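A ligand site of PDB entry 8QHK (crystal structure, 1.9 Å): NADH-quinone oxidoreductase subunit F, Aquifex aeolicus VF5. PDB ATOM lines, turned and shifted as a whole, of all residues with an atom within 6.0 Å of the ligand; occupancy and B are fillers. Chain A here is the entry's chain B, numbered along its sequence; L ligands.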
ATOM      1  N   ILE A 181     -21.146  19.773   2.737  1.00  0.00           N
ATOM      2  CA  ILE A 181     -21.283  21.161   3.140  1.00  0.00           C
ATOM      3  C   ILE A 181     -22.598  21.403   3.872  1.00  0.00           C
ATOM      4  O   ILE A 181     -22.711  22.396   4.591  1.00  0.00           O
ATOM      5  CB  ILE A 181     -21.122  22.107   1.933  1.00  0.00           C
ATOM      6  CG1 ILE A 181     -20.922  23.553   2.371  1.00  0.00           C
ATOM      7  CG2 ILE A 181     -22.288  21.992   0.958  1.00  0.00           C
ATOM      8  CD1 ILE A 181     -19.711  23.780   3.240  1.00  0.00           C
ATOM      9  N   HIS A 198     -25.918  26.237   0.403  1.00  0.00           N
ATOM     10  CA  HIS A 198     -24.927  27.308   0.321  1.00  0.00           C
ATOM     11  C   HIS A 198     -24.813  27.979   1.688  1.00  0.00           C
ATOM     12  O   HIS A 198     -25.780  28.572   2.176  1.00  0.00           O
ATOM     13  CB  HIS A 198     -25.287  28.299  -0.782  1.00  0.00           C
ATOM     14  CG  HIS A 198     -25.104  27.764  -2.158  1.00  0.00           C
ATOM     15  ND1 HIS A 198     -25.747  28.306  -3.244  1.00  0.00           N
ATOM     16  CD2 HIS A 198     -24.377  26.751  -2.642  1.00  0.00           C
ATOM     17  CE1 HIS A 198     -25.402  27.630  -4.341  1.00  0.00           C
ATOM     18  NE2 HIS A 198     -24.572  26.694  -4.002  1.00  0.00           N
ATOM     19  N   PRO A 199     -23.656  27.891   2.381  1.00  0.00           N
ATOM     20  CA  PRO A 199     -23.450  28.622   3.630  1.00  0.00           C
ATOM     21  C   PRO A 199     -23.780  30.103   3.490  1.00  0.00           C
ATOM     22  O   PRO A 199     -23.644  30.681   2.407  1.00  0.00           O
ATOM     23  CB  PRO A 199     -21.961  28.405   3.927  1.00  0.00           C
ATOM     24  CG  PRO A 199     -21.674  27.050   3.308  1.00  0.00           C
ATOM     25  CD  PRO A 199     -22.516  27.023   2.042  1.00  0.00           C
ATOM     26  N   GLU A 345     -16.252  18.624  -2.364  1.00  0.00           N
ATOM     27  CA  GLU A 345     -17.266  19.136  -1.436  1.00  0.00           C
ATOM     28  C   GLU A 345     -17.367  20.669  -1.394  1.00  0.00           C
ATOM     29  O   GLU A 345     -18.339  21.181  -0.839  1.00  0.00           O
ATOM     30  CB  GLU A 345     -17.019  18.575  -0.042  1.00  0.00           C
ATOM     31  CG  GLU A 345     -17.109  17.052   0.042  1.00  0.00           C
ATOM     32  CD  GLU A 345     -18.389  16.401  -0.448  1.00  0.00           C
ATOM     33  OE1 GLU A 345     -19.444  17.081  -0.520  1.00  0.00           O
ATOM     34  OE2 GLU A 345     -18.333  15.185  -0.758  1.00  0.00           O
ATOM     35  N   THR A 346     -16.406  21.424  -1.936  1.00  0.00           N
ATOM     36  CA  THR A 346     -16.570  22.877  -1.976  1.00  0.00           C
ATOM     37  C   THR A 346     -17.891  23.229  -2.685  1.00  0.00           C
ATOM     38  O   THR A 346     -18.212  22.657  -3.729  1.00  0.00           O
ATOM     39  CB  THR A 346     -15.389  23.593  -2.644  1.00  0.00           C
ATOM     40  OG1 THR A 346     -15.764  24.968  -2.756  1.00  0.00           O
ATOM     41  CG2 THR A 346     -15.031  23.038  -4.007  1.00  0.00           C
ATOM     42  N   CYS A 347     -18.652  24.166  -2.102  1.00  0.00           N
ATOM     43  CA  CYS A 347     -19.930  24.560  -2.700  1.00  0.00           C
ATOM     44  C   CYS A 347     -19.722  25.598  -3.821  1.00  0.00           C
ATOM     45  O   CYS A 347     -20.623  25.829  -4.616  1.00  0.00           O
ATOM     46  CB  CYS A 347     -20.904  25.050  -1.636  1.00  0.00           C
ATOM     47  SG  CYS A 347     -20.734  26.803  -1.203  1.00  0.00           S
ATOM     48  N   GLY A 348     -18.537  26.229  -3.863  1.00  0.00           N
ATOM     49  CA  GLY A 348     -18.137  27.050  -4.998  1.00  0.00           C
ATOM     50  C   GLY A 348     -18.669  28.481  -4.986  1.00  0.00           C
ATOM     51  O   GLY A 348     -18.488  29.195  -5.971  1.00  0.00           O
ATOM     52  N   GLN A 349     -19.293  28.921  -3.877  1.00  0.00           N
ATOM     53  CA  GLN A 349     -19.744  30.299  -3.725  1.00  0.00           C
ATOM     54  C   GLN A 349     -18.579  31.293  -3.734  1.00  0.00           C
ATOM     55  O   GLN A 349     -18.710  32.402  -4.247  1.00  0.00           O
ATOM     56  CB  GLN A 349     -20.410  30.535  -2.366  1.00  0.00           C
ATOM     57  CG  GLN A 349     -21.873  30.140  -2.258  1.00  0.00           C
ATOM     58  CD  GLN A 349     -22.453  30.736  -1.006  1.00  0.00           C
ATOM     59  OE1 GLN A 349     -23.067  31.807  -1.039  1.00  0.00           O
ATOM     60  NE2 GLN A 349     -22.187  30.092   0.127  1.00  0.00           N
ATOM     61  N   CYS A 350     -17.490  30.906  -3.054  1.00  0.00           N
ATOM     62  CA  CYS A 350     -16.319  31.762  -2.875  1.00  0.00           C
ATOM     63  C   CYS A 350     -15.243  31.325  -3.879  1.00  0.00           C
ATOM     64  O   CYS A 350     -15.003  30.131  -4.053  1.00  0.00           O
ATOM     65  CB  CYS A 350     -15.777  31.687  -1.446  1.00  0.00           C
ATOM     66  SG  CYS A 350     -17.048  31.588  -0.145  1.00  0.00           S
ATOM     67  N   THR A 351     -14.607  32.308  -4.536  1.00  0.00           N
ATOM     68  CA  THR A 351     -13.740  32.023  -5.673  1.00  0.00           C
ATOM     69  C   THR A 351     -12.476  31.286  -5.216  1.00  0.00           C
ATOM     70  O   THR A 351     -12.151  30.244  -5.780  1.00  0.00           O
ATOM     71  CB  THR A 351     -13.466  33.285  -6.499  1.00  0.00           C
ATOM     72  OG1 THR A 351     -14.673  33.634  -7.191  1.00  0.00           O
ATOM     73  CG2 THR A 351     -12.336  33.113  -7.498  1.00  0.00           C
ATOM     74  N   CYS A 353     -11.914  29.411  -2.659  1.00  0.00           N
ATOM     75  CA  CYS A 353     -12.310  28.075  -2.258  1.00  0.00           C
ATOM     76  C   CYS A 353     -12.671  27.246  -3.489  1.00  0.00           C
ATOM     77  O   CYS A 353     -12.222  26.097  -3.607  1.00  0.00           O
ATOM     78  CB  CYS A 353     -13.472  28.121  -1.272  1.00  0.00           C
ATOM     79  SG  CYS A 353     -13.996  26.492  -0.665  1.00  0.00           S
ATOM     80  N   ARG A 354     -13.451  27.822  -4.406  1.00  0.00           N
ATOM     81  CA  ARG A 354     -13.899  27.101  -5.592  1.00  0.00           C
ATOM     82  C   ARG A 354     -12.703  26.594  -6.399  1.00  0.00           C
ATOM     83  O   ARG A 354     -12.620  25.402  -6.720  1.00  0.00           O
ATOM     84  CB  ARG A 354     -14.796  27.987  -6.464  1.00  0.00           C
ATOM     85  CG  ARG A 354     -15.291  27.314  -7.739  1.00  0.00           C
ATOM     86  CD  ARG A 354     -16.203  28.204  -8.573  1.00  0.00           C
ATOM     87  NE  ARG A 354     -15.554  29.400  -9.077  1.00  0.00           N
ATOM     88  CZ  ARG A 354     -15.757  30.621  -8.598  1.00  0.00           C
ATOM     89  NH1 ARG A 354     -16.510  30.788  -7.518  1.00  0.00           N
ATOM     90  NH2 ARG A 354     -15.196  31.669  -9.187  1.00  0.00           N
ATOM     91  N   CYS A 357      -9.709  24.499  -4.024  1.00  0.00           N
ATOM     92  CA  CYS A 357      -9.978  23.095  -3.729  1.00  0.00           C
ATOM     93  C   CYS A 357      -9.761  22.236  -4.971  1.00  0.00           C
ATOM     94  O   CYS A 357      -9.205  21.138  -4.887  1.00  0.00           O
ATOM     95  CB  CYS A 357     -11.383  22.900  -3.168  1.00  0.00           C
ATOM     96  SG  CYS A 357     -11.563  23.513  -1.470  1.00  0.00           S
ATOM     97  N   THR A 390     -11.328  35.218   1.627  1.00  0.00           N
ATOM     98  CA  THR A 390     -12.699  35.610   1.295  1.00  0.00           C
ATOM     99  C   THR A 390     -13.734  34.526   1.614  1.00  0.00           C
ATOM    100  O   THR A 390     -14.916  34.725   1.344  1.00  0.00           O
ATOM    101  CB  THR A 390     -12.868  36.043  -0.180  1.00  0.00           C
ATOM    102  OG1 THR A 390     -13.005  34.895  -1.014  1.00  0.00           O
ATOM    103  CG2 THR A 390     -11.732  36.919  -0.669  1.00  0.00           C
ATOM    104  N   SER A 391     -13.306  33.390   2.198  1.00  0.00           N
ATOM    105  CA  SER A 391     -14.215  32.285   2.480  1.00  0.00           C
ATOM    106  C   SER A 391     -15.257  32.708   3.513  1.00  0.00           C
ATOM    107  O   SER A 391     -14.949  33.458   4.430  1.00  0.00           O
ATOM    108  CB  SER A 391     -13.446  31.057   2.928  1.00  0.00           C
ATOM    109  OG  SER A 391     -12.613  31.328   4.042  1.00  0.00           O
ATOM    110  N   ILE A 392     -16.502  32.226   3.370  1.00  0.00           N
ATOM    111  CA  ILE A 392     -17.561  32.580   4.321  1.00  0.00           C
ATOM    112  C   ILE A 392     -17.918  31.389   5.217  1.00  0.00           C
ATOM    113  O   ILE A 392     -18.880  31.485   5.980  1.00  0.00           O
ATOM    114  CB  ILE A 392     -18.796  33.174   3.611  1.00  0.00           C
ATOM    115  CG1 ILE A 392     -19.509  32.174   2.697  1.00  0.00           C
ATOM    116  CG2 ILE A 392     -18.417  34.441   2.847  1.00  0.00           C
ATOM    117  CD1 ILE A 392     -20.509  32.819   1.750  1.00  0.00           C
ATOM    118  N   CYS A 393     -17.162  30.274   5.130  1.00  0.00           N
ATOM    119  CA  CYS A 393     -17.385  29.134   6.015  1.00  0.00           C
ATOM    120  C   CYS A 393     -16.089  28.358   6.240  1.00  0.00           C
ATOM    121  O   CYS A 393     -15.056  28.598   5.608  1.00  0.00           O
ATOM    122  CB  CYS A 393     -18.503  28.211   5.505  1.00  0.00           C
ATOM    123  SG  CYS A 393     -17.969  26.788   4.523  1.00  0.00           S
ATOM    124  N   GLY A 394     -16.174  27.409   7.183  1.00  0.00           N
ATOM    125  CA  GLY A 394     -15.019  26.718   7.734  1.00  0.00           C
ATOM    126  C   GLY A 394     -14.334  25.769   6.744  1.00  0.00           C
ATOM    127  O   GLY A 394     -13.191  25.371   6.976  1.00  0.00           O
ATOM    128  N   LEU A 395     -15.034  25.379   5.663  1.00  0.00           N
ATOM    129  CA  LEU A 395     -14.447  24.482   4.680  1.00  0.00           C
ATOM    130  C   LEU A 395     -13.276  25.178   3.976  1.00  0.00           C
ATOM    131  O   LEU A 395     -12.176  24.635   3.922  1.00  0.00           O
ATOM    132  CB  LEU A 395     -15.524  24.025   3.691  1.00  0.00           C
ATOM    133  CG  LEU A 395     -15.102  22.884   2.758  1.00  0.00           C
ATOM    134  CD1 LEU A 395     -16.303  22.081   2.279  1.00  0.00           C
ATOM    135  CD2 LEU A 395     -14.306  23.421   1.564  1.00  0.00           C
ATOM    136  N   GLY A 396     -13.512  26.388   3.453  1.00  0.00           N
ATOM    137  CA  GLY A 396     -12.464  27.156   2.804  1.00  0.00           C
ATOM    138  C   GLY A 396     -11.348  27.515   3.778  1.00  0.00           C
ATOM    139  O   GLY A 396     -10.180  27.564   3.410  1.00  0.00           O
ATOM    140  N   ALA A 397     -11.736  27.714   5.038  1.00  0.00           N
ATOM    141  CA  ALA A 397     -10.796  28.046   6.097  1.00  0.00           C
ATOM    142  C   ALA A 397      -9.793  26.913   6.334  1.00  0.00           C
ATOM    143  O   ALA A 397      -8.653  27.183   6.693  1.00  0.00           O
ATOM    144  CB  ALA A 397     -11.543  28.423   7.365  1.00  0.00           C
HETATM  145 FE1  LIG L   1     -18.744  27.254  -0.150  1.00  0.00          FE
HETATM  146 FE2  LIG L   1     -16.008  27.080   0.211  1.00  0.00          FE
HETATM  147 FE3  LIG L   1     -17.651  27.511   2.388  1.00  0.00          FE
HETATM  148 FE4  LIG L   1     -17.251  29.505   0.501  1.00  0.00          FE
HETATM  149  S1  LIG L   1     -15.669  28.593   1.941  1.00  0.00           S
HETATM  150  S2  LIG L   1     -19.264  28.905   1.445  1.00  0.00           S
HETATM  151  S3  LIG L   1     -17.120  28.231  -1.466  1.00  0.00           S
HETATM  152  S4  LIG L   1     -17.581  25.631   0.977  1.00  0.00           S
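The backbone NH (N) of Cys 350 lies close to a sulfur (S3) of the ligand, at 3.1 Å. SG of Cys 350 binds FE4 of the ligand, 2.2 Å away. SG of Cys 353 binds FE2 of the ligand, 2.3 Å away. SG of Cys 393 binds FE3 of the ligand, at 2.3 Å. A sulfur (S4) of the ligand lies close to the backbone NH of Cys 347 (3.6 Å). FE1 of the ligand is bound by SG of Cys 347, at 2.3 Å. N of Gln 349 lies close to S3 of the ligand, 3.3 Å away. The side-chain amide nitrogen (NE2) of Gln 349 sits close to a sulfur (S2) of the ligand, at 3.4 Å. The backbone NH of Gly 348 sits close to a sulfur (S3) of the ligand (3.4 Å). The backbone NH (N) of Gly 396 sits close to a sulfur (S1) of the ligand, 3.4 Å away. A sulfur (S3) of the ligand sits close to the side-chain hydroxyl (OG1) of Thr 346 (3.8 Å).
The backbone NH (N) of Ile 392 sits close to the side-chain sulfur (SG) of Cys 350 (3.6 Å). SG of Cys 353 lies close to OG1 of Thr 346 (3.1 Å). SG of Cys 357 lies close to O of Cys 353, 3.4 Å away. The side-chain sulfur (SG) of Cys 393 sits close to the backbone NH (N) of Leu 395 (3.4 Å). The side-chain sulfur of Cys 347 lies close to the backbone NH of Gln 349 (3.7 Å). NE2 of Gln 349 lies within hydrogen-bond range of O of Pro 199, 2.8 Å away. The backbone NH (N) of Gly 348 lies within hydrogen-bond range of the side-chain hydroxyl (OG1) of Thr 346 (3.2 Å). O of Gly 348 sits at hydrogen-bond distance from NH1 of Arg 354, 3.0 Å away.
Ile 181 touches the ligand (CD1 to S4, 3.6 Å). Pro 199 touches the ligand. CB of Ser 391 touches S1 of the ligand, 3.5 Å away. Ile 392 touches the ligand. Leu 395 touches the ligand (CB to S4, 3.8 Å). Hydrophobic or aromatic side chains within 4 Å of the ligand: Ile 181, Pro 199, Ile 392 and Leu 395.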
